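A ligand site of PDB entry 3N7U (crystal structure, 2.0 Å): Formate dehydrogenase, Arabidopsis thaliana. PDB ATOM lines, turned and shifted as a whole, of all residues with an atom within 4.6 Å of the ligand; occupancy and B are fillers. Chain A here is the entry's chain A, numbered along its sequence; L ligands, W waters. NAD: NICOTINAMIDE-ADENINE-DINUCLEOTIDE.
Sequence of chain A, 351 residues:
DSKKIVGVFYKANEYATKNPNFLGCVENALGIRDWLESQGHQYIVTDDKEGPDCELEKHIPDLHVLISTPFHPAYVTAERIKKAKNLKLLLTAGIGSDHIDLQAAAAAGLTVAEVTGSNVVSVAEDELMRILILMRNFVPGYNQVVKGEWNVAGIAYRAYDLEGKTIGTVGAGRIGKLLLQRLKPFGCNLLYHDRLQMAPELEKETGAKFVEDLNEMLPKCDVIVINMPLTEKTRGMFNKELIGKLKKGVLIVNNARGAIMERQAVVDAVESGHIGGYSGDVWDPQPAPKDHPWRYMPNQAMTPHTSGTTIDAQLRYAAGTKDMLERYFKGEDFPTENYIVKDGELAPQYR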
ATOM      1  N   PHE A  71     -19.051  31.534   5.996  1.00  0.00           N
ATOM      2  CA  PHE A  71     -20.353  31.703   5.353  1.00  0.00           C
ATOM      3  C   PHE A  71     -20.265  32.326   3.944  1.00  0.00           C
ATOM      4  O   PHE A  71     -21.193  32.199   3.133  1.00  0.00           O
ATOM      5  CB  PHE A  71     -21.294  32.525   6.306  1.00  0.00           C
ATOM      6  CG  PHE A  71     -20.961  32.304   7.748  1.00  0.00           C
ATOM      7  CD1 PHE A  71     -21.394  31.132   8.413  1.00  0.00           C
ATOM      8  CD2 PHE A  71     -20.125  33.203   8.422  1.00  0.00           C
ATOM      9  CE1 PHE A  71     -20.980  30.865   9.760  1.00  0.00           C
ATOM     10  CE2 PHE A  71     -19.715  32.980   9.738  1.00  0.00           C
ATOM     11  CZ  PHE A  71     -20.162  31.782  10.423  1.00  0.00           C
ATOM     12  N   ILE A  95     -15.410  29.604  12.575  1.00  0.00           N
ATOM     13  CA  ILE A  95     -14.679  28.375  12.902  1.00  0.00           C
ATOM     14  C   ILE A  95     -14.626  27.497  11.657  1.00  0.00           C
ATOM     15  O   ILE A  95     -15.658  27.313  10.954  1.00  0.00           O
ATOM     16  CB  ILE A  95     -15.344  27.607  14.053  1.00  0.00           C
ATOM     17  CG1 ILE A  95     -15.237  28.384  15.368  1.00  0.00           C
ATOM     18  CG2 ILE A  95     -14.682  26.181  14.229  1.00  0.00           C
ATOM     19  CD1 ILE A  95     -15.958  27.720  16.556  1.00  0.00           C
ATOM     20  N   GLY A  96     -13.406  26.996  11.352  1.00  0.00           N
ATOM     21  CA  GLY A  96     -13.158  26.096  10.198  1.00  0.00           C
ATOM     22  C   GLY A  96     -12.407  26.852   9.102  1.00  0.00           C
ATOM     23  O   GLY A  96     -12.951  27.765   8.470  1.00  0.00           O
ATOM     24  N   ASP A  98     -10.612  25.512   6.401  1.00  0.00           N
ATOM     25  CA  ASP A  98     -10.409  24.672   5.225  1.00  0.00           C
ATOM     26  C   ASP A  98     -10.588  25.356   3.847  1.00  0.00           C
ATOM     27  O   ASP A  98     -10.280  24.761   2.801  1.00  0.00           O
ATOM     28  CB  ASP A  98     -11.430  23.518   5.341  1.00  0.00           C
ATOM     29  CG  ASP A  98     -12.852  24.048   5.581  1.00  0.00           C
ATOM     30  OD1 ASP A  98     -13.237  24.201   6.750  1.00  0.00           O
ATOM     31  OD2 ASP A  98     -13.547  24.329   4.575  1.00  0.00           O
ATOM     32  N   ASN A 119     -18.913  29.933  18.082  1.00  0.00           N
ATOM     33  CA  ASN A 119     -20.275  29.621  17.653  1.00  0.00           C
ATOM     34  C   ASN A 119     -20.662  28.110  17.858  1.00  0.00           C
ATOM     35  O   ASN A 119     -21.584  27.619  17.240  1.00  0.00           O
ATOM     36  CB  ASN A 119     -20.486  30.117  16.191  1.00  0.00           C
ATOM     37  CG  ASN A 119     -19.502  29.490  15.178  1.00  0.00           C
ATOM     38  OD1 ASN A 119     -18.852  28.489  15.497  1.00  0.00           O
ATOM     39  ND2 ASN A 119     -19.408  30.063  13.938  1.00  0.00           N
ATOM     40  N   VAL A 120     -19.914  27.407  18.730  1.00  0.00           N
ATOM     41  CA  VAL A 120     -20.122  25.972  18.938  1.00  0.00           C
ATOM     42  C   VAL A 120     -21.500  25.639  19.569  1.00  0.00           C
ATOM     43  O   VAL A 120     -22.162  24.667  19.165  1.00  0.00           O
ATOM     44  CB  VAL A 120     -18.944  25.309  19.739  1.00  0.00           C
ATOM     45  CG1 VAL A 120     -17.630  25.380  18.949  1.00  0.00           C
ATOM     46  CG2 VAL A 120     -18.756  25.952  21.131  1.00  0.00           C
ATOM     47  N   VAL A 123     -24.199  25.969  16.650  1.00  0.00           N
ATOM     48  CA  VAL A 123     -24.259  24.814  15.717  1.00  0.00           C
ATOM     49  C   VAL A 123     -24.898  23.601  16.452  1.00  0.00           C
ATOM     50  O   VAL A 123     -25.702  22.892  15.886  1.00  0.00           O
ATOM     51  CB  VAL A 123     -22.842  24.436  15.138  1.00  0.00           C
ATOM     52  CG1 VAL A 123     -22.933  23.316  14.072  1.00  0.00           C
ATOM     53  CG2 VAL A 123     -22.149  25.659  14.519  1.00  0.00           C
ATOM     54  N   ALA A 172     -16.588  14.009  18.194  1.00  0.00           N
ATOM     55  CA  ALA A 172     -17.049  14.492  19.491  1.00  0.00           C
ATOM     56  C   ALA A 172     -16.047  15.513  20.043  1.00  0.00           C
ATOM     57  O   ALA A 172     -15.466  15.328  21.137  1.00  0.00           O
ATOM     58  CB  ALA A 172     -17.251  13.338  20.486  1.00  0.00           C
ATOM     59  N   GLY A 173     -15.883  16.611  19.308  1.00  0.00           N
ATOM     60  CA  GLY A 173     -15.133  17.759  19.829  1.00  0.00           C
ATOM     61  C   GLY A 173     -16.069  18.688  20.559  1.00  0.00           C
ATOM     62  O   GLY A 173     -17.001  18.246  21.247  1.00  0.00           O
ATOM     63  N   ARG A 174     -15.833  20.000  20.427  1.00  0.00           N
ATOM     64  CA  ARG A 174     -16.607  21.005  21.134  1.00  0.00           C
ATOM     65  C   ARG A 174     -18.109  20.912  20.770  1.00  0.00           C
ATOM     66  O   ARG A 174     -18.957  20.816  21.656  1.00  0.00           O
ATOM     67  CB  ARG A 174     -16.051  22.404  20.807  1.00  0.00           C
ATOM     68  CG  ARG A 174     -14.644  22.583  21.403  1.00  0.00           C
ATOM     69  CD  ARG A 174     -14.037  23.949  21.136  1.00  0.00           C
ATOM     70  NE  ARG A 174     -12.732  24.064  21.781  1.00  0.00           N
ATOM     71  CZ  ARG A 174     -11.603  23.543  21.294  1.00  0.00           C
ATOM     72  NH1 ARG A 174     -11.591  22.844  20.157  1.00  0.00           N
ATOM     73  NH2 ARG A 174     -10.465  23.759  21.959  1.00  0.00           N
ATOM     74  N   ILE A 175     -18.396  20.881  19.472  1.00  0.00           N
ATOM     75  CA  ILE A 175     -19.801  20.870  19.021  1.00  0.00           C
ATOM     76  C   ILE A 175     -20.494  19.540  19.370  1.00  0.00           C
ATOM     77  O   ILE A 175     -21.615  19.539  19.895  1.00  0.00           O
ATOM     78  CB  ILE A 175     -19.954  21.187  17.500  1.00  0.00           C
ATOM     79  CG1 ILE A 175     -19.466  22.616  17.215  1.00  0.00           C
ATOM     80  CG2 ILE A 175     -21.424  21.012  17.047  1.00  0.00           C
ATOM     81  CD1 ILE A 175     -19.301  22.925  15.726  1.00  0.00           C
ATOM     82  N   GLY A 176     -19.803  18.423  19.097  1.00  0.00           N
ATOM     83  CA  GLY A 176     -20.389  17.077  19.340  1.00  0.00           C
ATOM     84  C   GLY A 176     -20.718  16.892  20.811  1.00  0.00           C
ATOM     85  O   GLY A 176     -21.769  16.347  21.161  1.00  0.00           O
ATOM     86  N   HIS A 193     -18.221   8.291  17.758  1.00  0.00           N
ATOM     87  CA  HIS A 193     -16.883   7.942  17.258  1.00  0.00           C
ATOM     88  C   HIS A 193     -16.002   9.215  17.200  1.00  0.00           C
ATOM     89  O   HIS A 193     -16.475  10.303  16.812  1.00  0.00           O
ATOM     90  CB  HIS A 193     -16.986   7.314  15.874  1.00  0.00           C
ATOM     91  CG  HIS A 193     -15.668   7.201  15.173  1.00  0.00           C
ATOM     92  ND1 HIS A 193     -14.728   6.245  15.494  1.00  0.00           N
ATOM     93  CD2 HIS A 193     -15.111   7.963  14.189  1.00  0.00           C
ATOM     94  CE1 HIS A 193     -13.658   6.411  14.736  1.00  0.00           C
ATOM     95  NE2 HIS A 193     -13.866   7.440  13.935  1.00  0.00           N
ATOM     96  N   ASP A 194     -14.753   9.085  17.644  1.00  0.00           N
ATOM     97  CA  ASP A 194     -13.720  10.123  17.491  1.00  0.00           C
ATOM     98  C   ASP A 194     -12.367   9.387  17.589  1.00  0.00           C
ATOM     99  O   ASP A 194     -12.324   8.215  18.047  1.00  0.00           O
ATOM    100  CB  ASP A 194     -13.831  11.167  18.616  1.00  0.00           C
ATOM    101  CG  ASP A 194     -13.112  12.499  18.280  1.00  0.00           C
ATOM    102  OD1 ASP A 194     -11.861  12.527  18.363  1.00  0.00           O
ATOM    103  OD2 ASP A 194     -13.817  13.514  17.951  1.00  0.00           O
ATOM    104  N   ARG A 195     -11.285  10.039  17.159  1.00  0.00           N
ATOM    105  CA  ARG A 195      -9.931   9.578  17.497  1.00  0.00           C
ATOM    106  C   ARG A 195      -9.678   9.715  18.989  1.00  0.00           C
ATOM    107  O   ARG A 195      -8.839   9.011  19.556  1.00  0.00           O
ATOM    108  CB  ARG A 195      -8.853  10.305  16.685  1.00  0.00           C
ATOM    109  CG  ARG A 195      -9.093  10.168  15.188  1.00  0.00           C
ATOM    110  CD  ARG A 195      -7.928  10.600  14.308  1.00  0.00           C
ATOM    111  NE  ARG A 195      -7.589  12.015  14.465  1.00  0.00           N
ATOM    112  CZ  ARG A 195      -7.002  12.748  13.527  1.00  0.00           C
ATOM    113  NH1 ARG A 195      -6.738  14.043  13.741  1.00  0.00           N
ATOM    114  NH2 ARG A 195      -6.708  12.216  12.351  1.00  0.00           N
ATOM    115  N   LEU A 196     -10.437  10.588  19.665  1.00  0.00           N
ATOM    116  CA  LEU A 196     -10.227  10.821  21.078  1.00  0.00           C
ATOM    117  C   LEU A 196     -11.472  10.539  21.907  1.00  0.00           C
ATOM    118  O   LEU A 196     -12.546  11.090  21.630  1.00  0.00           O
ATOM    119  CB  LEU A 196      -9.779  12.273  21.317  1.00  0.00           C
ATOM    120  CG  LEU A 196      -8.591  12.802  20.510  1.00  0.00           C
ATOM    121  CD1 LEU A 196      -8.541  14.337  20.613  1.00  0.00           C
ATOM    122  CD2 LEU A 196      -7.262  12.178  21.008  1.00  0.00           C
ATOM    123  N   ASN A 227     -19.576  15.832  12.641  1.00  0.00           N
ATOM    124  CA  ASN A 227     -18.998  16.789  13.616  1.00  0.00           C
ATOM    125  C   ASN A 227     -17.462  16.767  13.674  1.00  0.00           C
ATOM    126  O   ASN A 227     -16.889  16.862  14.761  1.00  0.00           O
ATOM    127  CB  ASN A 227     -19.614  16.606  15.011  1.00  0.00           C
ATOM    128  CG  ASN A 227     -20.913  17.424  15.212  1.00  0.00           C
ATOM    129  OD1 ASN A 227     -20.969  18.602  14.847  1.00  0.00           O
ATOM    130  ND2 ASN A 227     -21.936  16.795  15.792  1.00  0.00           N
ATOM    131  N   MET A 228     -16.819  16.679  12.501  1.00  0.00           N
ATOM    132  CA  MET A 228     -15.353  16.799  12.339  1.00  0.00           C
ATOM    133  C   MET A 228     -14.955  17.988  11.440  1.00  0.00           C
ATOM    134  O   MET A 228     -15.795  18.419  10.655  1.00  0.00           O
ATOM    135  CB  MET A 228     -14.776  15.513  11.697  1.00  0.00           C
ATOM    136  CG  MET A 228     -14.982  14.195  12.561  1.00  0.00           C
ATOM    137  SD  MET A 228     -14.591  12.690  11.595  1.00  0.00           S
ATOM    138  CE  MET A 228     -15.624  12.741  10.170  1.00  0.00           C
ATOM    139  N   PRO A 229     -13.696  18.480  11.506  1.00  0.00           N
ATOM    140  CA  PRO A 229     -13.304  19.480  10.491  1.00  0.00           C
ATOM    141  C   PRO A 229     -13.150  18.848   9.115  1.00  0.00           C
ATOM    142  O   PRO A 229     -13.171  17.584   9.002  1.00  0.00           O
ATOM    143  CB  PRO A 229     -11.923  19.978  10.964  1.00  0.00           C
ATOM    144  CG  PRO A 229     -11.735  19.429  12.354  1.00  0.00           C
ATOM    145  CD  PRO A 229     -12.555  18.164  12.394  1.00  0.00           C
ATOM    146  N   LEU A 230     -13.056  19.692   8.071  1.00  0.00           N
ATOM    147  CA  LEU A 230     -12.736  19.249   6.714  1.00  0.00           C
ATOM    148  C   LEU A 230     -11.200  19.174   6.637  1.00  0.00           C
ATOM    149  O   LEU A 230     -10.537  20.189   6.670  1.00  0.00           O
ATOM    150  CB  LEU A 230     -13.299  20.191   5.627  1.00  0.00           C
ATOM    151  CG  LEU A 230     -12.902  19.991   4.157  1.00  0.00           C
ATOM    152  CD1 LEU A 230     -13.148  18.585   3.655  1.00  0.00           C
ATOM    153  CD2 LEU A 230     -13.613  20.982   3.233  1.00  0.00           C
ATOM    154  N   LYS A 233      -7.850  13.834   5.574  1.00  0.00           N
ATOM    155  CA  LYS A 233      -8.479  12.550   5.870  1.00  0.00           C
ATOM    156  C   LYS A 233     -10.035  12.502   5.745  1.00  0.00           C
ATOM    157  O   LYS A 233     -10.597  11.518   5.216  1.00  0.00           O
ATOM    158  CB  LYS A 233      -8.006  12.066   7.246  1.00  0.00           C
ATOM    159  CG  LYS A 233      -6.604  11.456   7.209  1.00  0.00           C
ATOM    160  CD  LYS A 233      -6.081  11.281   8.621  1.00  0.00           C
ATOM    161  CE  LYS A 233      -4.625  10.719   8.611  1.00  0.00           C
ATOM    162  NZ  LYS A 233      -4.121  10.696  10.039  1.00  0.00           N
ATOM    163  N   THR A 234     -10.725  13.548   6.238  1.00  0.00           N
ATOM    164  CA  THR A 234     -12.218  13.596   6.150  1.00  0.00           C
ATOM    165  C   THR A 234     -12.786  13.962   4.774  1.00  0.00           C
ATOM    166  O   THR A 234     -13.924  13.616   4.477  1.00  0.00           O
ATOM    167  CB  THR A 234     -12.857  14.504   7.232  1.00  0.00           C
ATOM    168  OG1 THR A 234     -12.503  15.873   6.988  1.00  0.00           O
ATOM    169  CG2 THR A 234     -12.373  14.083   8.644  1.00  0.00           C
ATOM    170  N   ASN A 255     -23.878  19.917   9.520  1.00  0.00           N
ATOM    171  CA  ASN A 255     -23.500  21.318   9.659  1.00  0.00           C
ATOM    172  C   ASN A 255     -21.974  21.460   9.854  1.00  0.00           C
ATOM    173  O   ASN A 255     -21.524  22.472  10.385  1.00  0.00           O
ATOM    174  CB  ASN A 255     -24.243  22.013  10.860  1.00  0.00           C
ATOM    175  CG  ASN A 255     -25.723  22.347  10.563  1.00  0.00           C
ATOM    176  OD1 ASN A 255     -26.345  21.743   9.679  1.00  0.00           O
ATOM    177  ND2 ASN A 255     -26.329  23.272  11.365  1.00  0.00           N
ATOM    178  N   ALA A 256     -21.191  20.466   9.419  1.00  0.00           N
ATOM    179  CA  ALA A 256     -19.744  20.526   9.553  1.00  0.00           C
ATOM    180  C   ALA A 256     -19.147  21.184   8.307  1.00  0.00           C
ATOM    181  O   ALA A 256     -18.901  22.397   8.330  1.00  0.00           O
ATOM    182  CB  ALA A 256     -19.143  19.095   9.792  1.00  0.00           C
ATOM    183  N   ARG A 257     -18.925  20.389   7.235  1.00  0.00           N
ATOM    184  CA  ARG A 257     -18.541  20.902   5.924  1.00  0.00           C
ATOM    185  C   ARG A 257     -19.091  19.967   4.858  1.00  0.00           C
ATOM    186  O   ARG A 257     -19.114  18.742   5.051  1.00  0.00           O
ATOM    187  CB  ARG A 257     -17.013  21.013   5.749  1.00  0.00           C
ATOM    188  CG  ARG A 257     -16.343  22.121   6.537  1.00  0.00           C
ATOM    189  CD  ARG A 257     -16.753  23.498   6.086  1.00  0.00           C
ATOM    190  NE  ARG A 257     -16.088  24.590   6.795  1.00  0.00           N
ATOM    191  CZ  ARG A 257     -16.622  25.299   7.797  1.00  0.00           C
ATOM    192  NH1 ARG A 257     -17.808  24.990   8.314  1.00  0.00           N
ATOM    193  NH2 ARG A 257     -15.939  26.302   8.333  1.00  0.00           N
ATOM    194  N   ASP A 281     -26.505  22.990   6.660  1.00  0.00           N
ATOM    195  CA  ASP A 281     -26.313  24.380   6.203  1.00  0.00           C
ATOM    196  C   ASP A 281     -25.029  24.580   5.372  1.00  0.00           C
ATOM    197  O   ASP A 281     -24.833  25.677   4.887  1.00  0.00           O
ATOM    198  CB  ASP A 281     -26.365  25.370   7.413  1.00  0.00           C
ATOM    199  CG  ASP A 281     -25.174  25.196   8.389  1.00  0.00           C
ATOM    200  OD1 ASP A 281     -24.510  24.154   8.375  1.00  0.00           O
ATOM    201  OD2 ASP A 281     -24.864  26.128   9.186  1.00  0.00           O
ATOM    202  N   VAL A 282     -24.210  23.538   5.174  1.00  0.00           N
ATOM    203  CA  VAL A 282     -22.879  23.669   4.482  1.00  0.00           C
ATOM    204  C   VAL A 282     -22.768  22.953   3.131  1.00  0.00           C
ATOM    205  O   VAL A 282     -23.304  21.870   2.959  1.00  0.00           O
ATOM    206  CB  VAL A 282     -21.717  23.218   5.380  1.00  0.00           C
ATOM    207  CG1 VAL A 282     -21.525  24.206   6.473  1.00  0.00           C
ATOM    208  CG2 VAL A 282     -21.966  21.794   5.955  1.00  0.00           C
ATOM    209  N   HIS A 305     -25.642  28.711   4.410  1.00  0.00           N
ATOM    210  CA  HIS A 305     -24.713  28.588   5.544  1.00  0.00           C
ATOM    211  C   HIS A 305     -24.961  29.639   6.619  1.00  0.00           C
ATOM    212  O   HIS A 305     -24.344  30.711   6.585  1.00  0.00           O
ATOM    213  CB  HIS A 305     -23.220  28.553   5.034  1.00  0.00           C
ATOM    214  CG  HIS A 305     -22.217  28.234   6.111  1.00  0.00           C
ATOM    215  ND1 HIS A 305     -20.862  28.203   5.879  1.00  0.00           N
ATOM    216  CD2 HIS A 305     -22.367  27.925   7.420  1.00  0.00           C
ATOM    217  CE1 HIS A 305     -20.224  27.919   7.002  1.00  0.00           C
ATOM    218  NE2 HIS A 305     -21.119  27.745   7.948  1.00  0.00           N
ATOM    219  N   SER A 307     -25.809  28.653  10.427  1.00  0.00           N
ATOM    220  CA  SER A 307     -25.946  28.240  11.857  1.00  0.00           C
ATOM    221  C   SER A 307     -24.903  28.900  12.754  1.00  0.00           C
ATOM    222  O   SER A 307     -25.194  29.270  13.906  1.00  0.00           O
ATOM    223  CB  SER A 307     -26.034  26.709  12.063  1.00  0.00           C
ATOM    224  OG  SER A 307     -24.797  26.045  11.708  1.00  0.00           O
ATOM    225  N   GLY A 308     -23.692  29.095  12.219  1.00  0.00           N
ATOM    226  CA  GLY A 308     -22.607  29.774  12.975  1.00  0.00           C
ATOM    227  C   GLY A 308     -22.597  31.307  12.894  1.00  0.00           C
ATOM    228  O   GLY A 308     -21.641  31.940  13.376  1.00  0.00           O
ATOM    229  N   GLN A 349      -6.072  18.423  15.262  1.00  0.00           N
ATOM    230  CA  GLN A 349      -7.373  17.973  14.785  1.00  0.00           C
ATOM    231  C   GLN A 349      -7.473  18.035  13.274  1.00  0.00           C
ATOM    232  O   GLN A 349      -8.391  17.458  12.707  1.00  0.00           O
ATOM    233  CB  GLN A 349      -8.526  18.759  15.441  1.00  0.00           C
ATOM    234  CG  GLN A 349      -8.560  20.256  15.027  1.00  0.00           C
ATOM    235  CD  GLN A 349      -7.766  21.189  15.953  1.00  0.00           C
ATOM    236  OE1 GLN A 349      -6.772  20.805  16.599  1.00  0.00           O
ATOM    237  NE2 GLN A 349      -8.173  22.440  15.969  1.00  0.00           N
ATOM    238  N   TYR A 350      -6.552  18.763  12.615  1.00  0.00           N
ATOM    239  CA  TYR A 350      -6.499  18.715  11.152  1.00  0.00           C
ATOM    240  C   TYR A 350      -5.533  17.653  10.592  1.00  0.00           C
ATOM    241  O   TYR A 350      -5.561  17.364   9.407  1.00  0.00           O
ATOM    242  CB  TYR A 350      -6.178  20.122  10.569  1.00  0.00           C
ATOM    243  CG  TYR A 350      -7.398  21.058  10.568  1.00  0.00           C
ATOM    244  CD1 TYR A 350      -7.805  21.690  11.724  1.00  0.00           C
ATOM    245  CD2 TYR A 350      -8.144  21.264   9.405  1.00  0.00           C
ATOM    246  CE1 TYR A 350      -8.917  22.545  11.729  1.00  0.00           C
ATOM    247  CE2 TYR A 350      -9.275  22.138   9.401  1.00  0.00           C
ATOM    248  CZ  TYR A 350      -9.642  22.760  10.584  1.00  0.00           C
ATOM    249  OH  TYR A 350     -10.756  23.591  10.627  1.00  0.00           O
HETATM  250  PA  NAD L   1     -13.186  20.529  17.373  1.00  0.00           P
HETATM  251  O1A NAD L   1     -11.788  20.705  16.834  1.00  0.00           O
HETATM  252  O2A NAD L   1     -13.335  20.974  18.793  1.00  0.00           O
HETATM  253  O5B NAD L   1     -13.573  18.975  17.173  1.00  0.00           O
HETATM  254  C5B NAD L   1     -13.164  18.280  15.977  1.00  0.00           C
HETATM  255  C4B NAD L   1     -13.046  16.780  16.352  1.00  0.00           C
HETATM  256  O4B NAD L   1     -12.775  16.012  15.161  1.00  0.00           O
HETATM  257  C3B NAD L   1     -11.919  16.514  17.335  1.00  0.00           C
HETATM  258  O3B NAD L   1     -12.462  15.972  18.572  1.00  0.00           O
HETATM  259  C2B NAD L   1     -10.974  15.557  16.539  1.00  0.00           C
HETATM  260  O2B NAD L   1     -10.396  14.580  17.381  1.00  0.00           O
HETATM  261  C1B NAD L   1     -11.899  14.909  15.506  1.00  0.00           C
HETATM  262  N9A NAD L   1     -11.266  14.412  14.278  1.00  0.00           N
HETATM  263  C8A NAD L   1     -10.455  15.092  13.402  1.00  0.00           C
HETATM  264  N7A NAD L   1     -10.127  14.294  12.402  1.00  0.00           N
HETATM  265  C5A NAD L   1     -10.753  13.087  12.599  1.00  0.00           C
HETATM  266  C6A NAD L   1     -10.763  11.856  11.922  1.00  0.00           C
HETATM  267  N6A NAD L   1     -10.068  11.730  10.743  1.00  0.00           N
HETATM  268  N1A NAD L   1     -11.514  10.854  12.405  1.00  0.00           N
HETATM  269  C2A NAD L   1     -12.206  10.974  13.549  1.00  0.00           C
HETATM  270  N3A NAD L   1     -12.180  12.104  14.246  1.00  0.00           N
HETATM  271  C4A NAD L   1     -11.469  13.150  13.801  1.00  0.00           C
HETATM  272  O3  NAD L   1     -14.184  21.321  16.361  1.00  0.00           O
HETATM  273  PN  NAD L   1     -15.646  21.954  16.665  1.00  0.00           P
HETATM  274  O1N NAD L   1     -15.594  23.267  17.470  1.00  0.00           O
HETATM  275  O2N NAD L   1     -16.523  20.769  17.183  1.00  0.00           O
HETATM  276  O5D NAD L   1     -16.077  22.156  15.153  1.00  0.00           O
HETATM  277  C5D NAD L   1     -15.975  21.078  14.218  1.00  0.00           C
HETATM  278  C4D NAD L   1     -16.142  21.589  12.800  1.00  0.00           C
HETATM  279  O4D NAD L   1     -17.505  22.020  12.522  1.00  0.00           O
HETATM  280  C3D NAD L   1     -15.253  22.800  12.405  1.00  0.00           C
HETATM  281  O3D NAD L   1     -13.954  22.366  11.961  1.00  0.00           O
HETATM  282  C2D NAD L   1     -16.034  23.443  11.233  1.00  0.00           C
HETATM  283  O2D NAD L   1     -15.542  22.875  10.001  1.00  0.00           O
HETATM  284  C1D NAD L   1     -17.528  22.999  11.469  1.00  0.00           C
HETATM  285  N1N NAD L   1     -18.291  24.189  11.907  1.00  0.00           N
HETATM  286  C2N NAD L   1     -19.396  24.554  11.217  1.00  0.00           C
HETATM  287  C3N NAD L   1     -20.121  25.728  11.593  1.00  0.00           C
HETATM  288  C7N NAD L   1     -21.342  26.195  10.851  1.00  0.00           C
HETATM  289  O7N NAD L   1     -21.656  27.394  10.876  1.00  0.00           O
HETATM  290  N7N NAD L   1     -22.084  25.351  10.107  1.00  0.00           N
HETATM  291  C4N NAD L   1     -19.634  26.471  12.682  1.00  0.00           C
HETATM  292  C5N NAD L   1     -18.516  26.052  13.407  1.00  0.00           C
HETATM  293  C6N NAD L   1     -17.854  24.895  12.980  1.00  0.00           C
HETATM  294  O   HOH W   1     -11.410  16.890  20.751  1.00  0.00           O
HETATM  295  O   HOH W   2      -9.684  20.363  18.522  1.00  0.00           O
HETATM  296  O   HOH W   3     -10.964  23.031  15.296  1.00  0.00           O
HETATM  297  O   HOH W   4     -13.073  22.562   8.982  1.00  0.00           O
HETATM  298  O   HOH W   5     -12.027   8.033  12.159  1.00  0.00           O
HETATM  299  O   HOH W   6     -14.082  25.362  17.894  1.00  0.00           O
HETATM  300  O   HOH W   7     -17.146  18.118  17.131  1.00  0.00           O
HETATM  301  O   HOH W   8      -8.037  14.277  16.523  1.00  0.00           O
HETATM  302  O   HOH W   9     -12.201  19.602  21.019  1.00  0.00           O
HETATM  303  O   HOH W  10      -8.439  14.361  10.150  1.00  0.00           O
HETATM  304  O   HOH W  11      -9.781   8.907   9.174  1.00  0.00           O
HETATM  305  O   HOH W  12     -11.693  24.061  12.902  1.00  0.00           O
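The backbone NH (N) of Leu 196 sits at hydrogen-bond distance from the side-chain carboxylate (OD1) of Asp 194 (2.7 Å).
The backbone NH of Ala 172 sits at hydrogen-bond distance from the side-chain carboxylate of Asp 194, 2.8 Å away.
OD1 of Asn 255 is in hydrogen-bond range of N of Asp 281 (3.3 Å).
O of Asp 281 sits close to N of His 305.
OD2 of Asp 281 lies within hydrogen-bond range of OG of Ser 307.
O of Pro 229 sits at hydrogen-bond distance from OG1 of Thr 234 (2.7 Å).
The guanidinium group of Arg 257 lies within hydrogen-bond range of the backbone carbonyl oxygen of Ile 95.
The guanidinium group (NE) of Arg 257 lies within salt-bridge range of the side-chain carboxylate (OD1) of Asp 98, 2.9 Å away.
An oxygen (O2B) of the ligand sits at hydrogen-bond distance from the side-chain carboxylate (OD1) of Asp 194.
N of Arg 174 sits at hydrogen-bond distance from O2A of the ligand (3.1 Å).
O2A of the ligand is in salt-bridge range of NH1 of Arg 174, 2.9 Å away.
O of Asn 255 is in hydrogen-bond range of N7N of the ligand, 2.9 Å away.
The backbone NH (N) of Ile 175 lies within hydrogen-bond range of an oxygen (O2N) of the ligand.
O7N of the ligand lies within hydrogen-bond range of N of Gly 308 (3.0 Å).
A ring nitrogen (NE2) of His 305 is in hydrogen-bond range of an oxygen (O7N) of the ligand (3.0 Å).
The side-chain carboxylate (OD2) of Asp 281 lies within hydrogen-bond range of a nitrogen (N7N) of the ligand (3.0 Å).
OG of Ser 307 is in hydrogen-bond range of N7N of the ligand (3.2 Å).
N3A of the ligand lies close to SD of Met 228.
Phe 71 touches the ligand (CE1 to O7N, 3.7 Å).
CB of Ile 95 touches C5N of the ligand, at 3.6 Å.
OD1 of Asn 119 touches C5N of the ligand (3.2 Å).
CG1 of Val 120 touches O1N of the ligand (3.3 Å).
Val 123 touches the ligand.
C of Ala 172 touches O3B of the ligand, at 3.9 Å.
Gly 173 touches the ligand.
NE2 of His 193 touches C2A of the ligand (3.9 Å).
Arg 195 touches the ligand.
Leu 196 touches the ligand.
Pro 229 touches the ligand.
CG2 of Thr 234 touches N6A of the ligand, 3.9 Å away.
O of Ala 256 touches C1D of the ligand, at 3.5 Å.
Arg 257 touches the ligand.
CG1 of Val 282 touches N7N of the ligand (3.9 Å).
Gln 349 touches the ligand (O to C8A, 3.2 Å).
Tyr 350 touches the ligand (OH to O3D, 3.7 Å).
Hydrophobic or aromatic side chains within 4 Å of the ligand: Phe 71, Ile 95, Val 120, Val 123, Ile 175, Leu 196, Met 228, Pro 229, Val 282 and His 305.
Of the 32 residues printed, 26 come within 4 Å of the ligand.
Water W4 lies within hydrogen-bond range of an oxygen (O2D) of the ligand (2.7 Å), the side-chain carboxylate of Asp 98 (2.8 Å), the backbone NH of Leu 230 (3.0 Å) and the side-chain hydroxyl of Tyr 350 (3.0 Å).
Water W7 lies within hydrogen-bond range of the backbone carbonyl oxygen of Asn 227 (2.7 Å), an oxygen (O2N) of the ligand (2.7 Å), the backbone NH of Gly 173 (2.9 Å) and the backbone NH of Gly 176 (3.3 Å).
Water W9 lies within hydrogen-bond range of O2A of the ligand (2.9 Å) and NH1 of Arg 174 (3.4 Å).
Water W5 lies within hydrogen-bond range of NE2 of His 193 (2.6 Å) and N1A of the ligand (2.9 Å).
Water W3 bridges an oxygen (O1A) of the ligand (2.9 Å) and the side-chain amide nitrogen of Gln 349 (2.9 Å).
Water W12 bridges the side-chain hydroxyl of Tyr 350 (2.5 Å) and an oxygen (O3D) of the ligand (3.0 Å).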
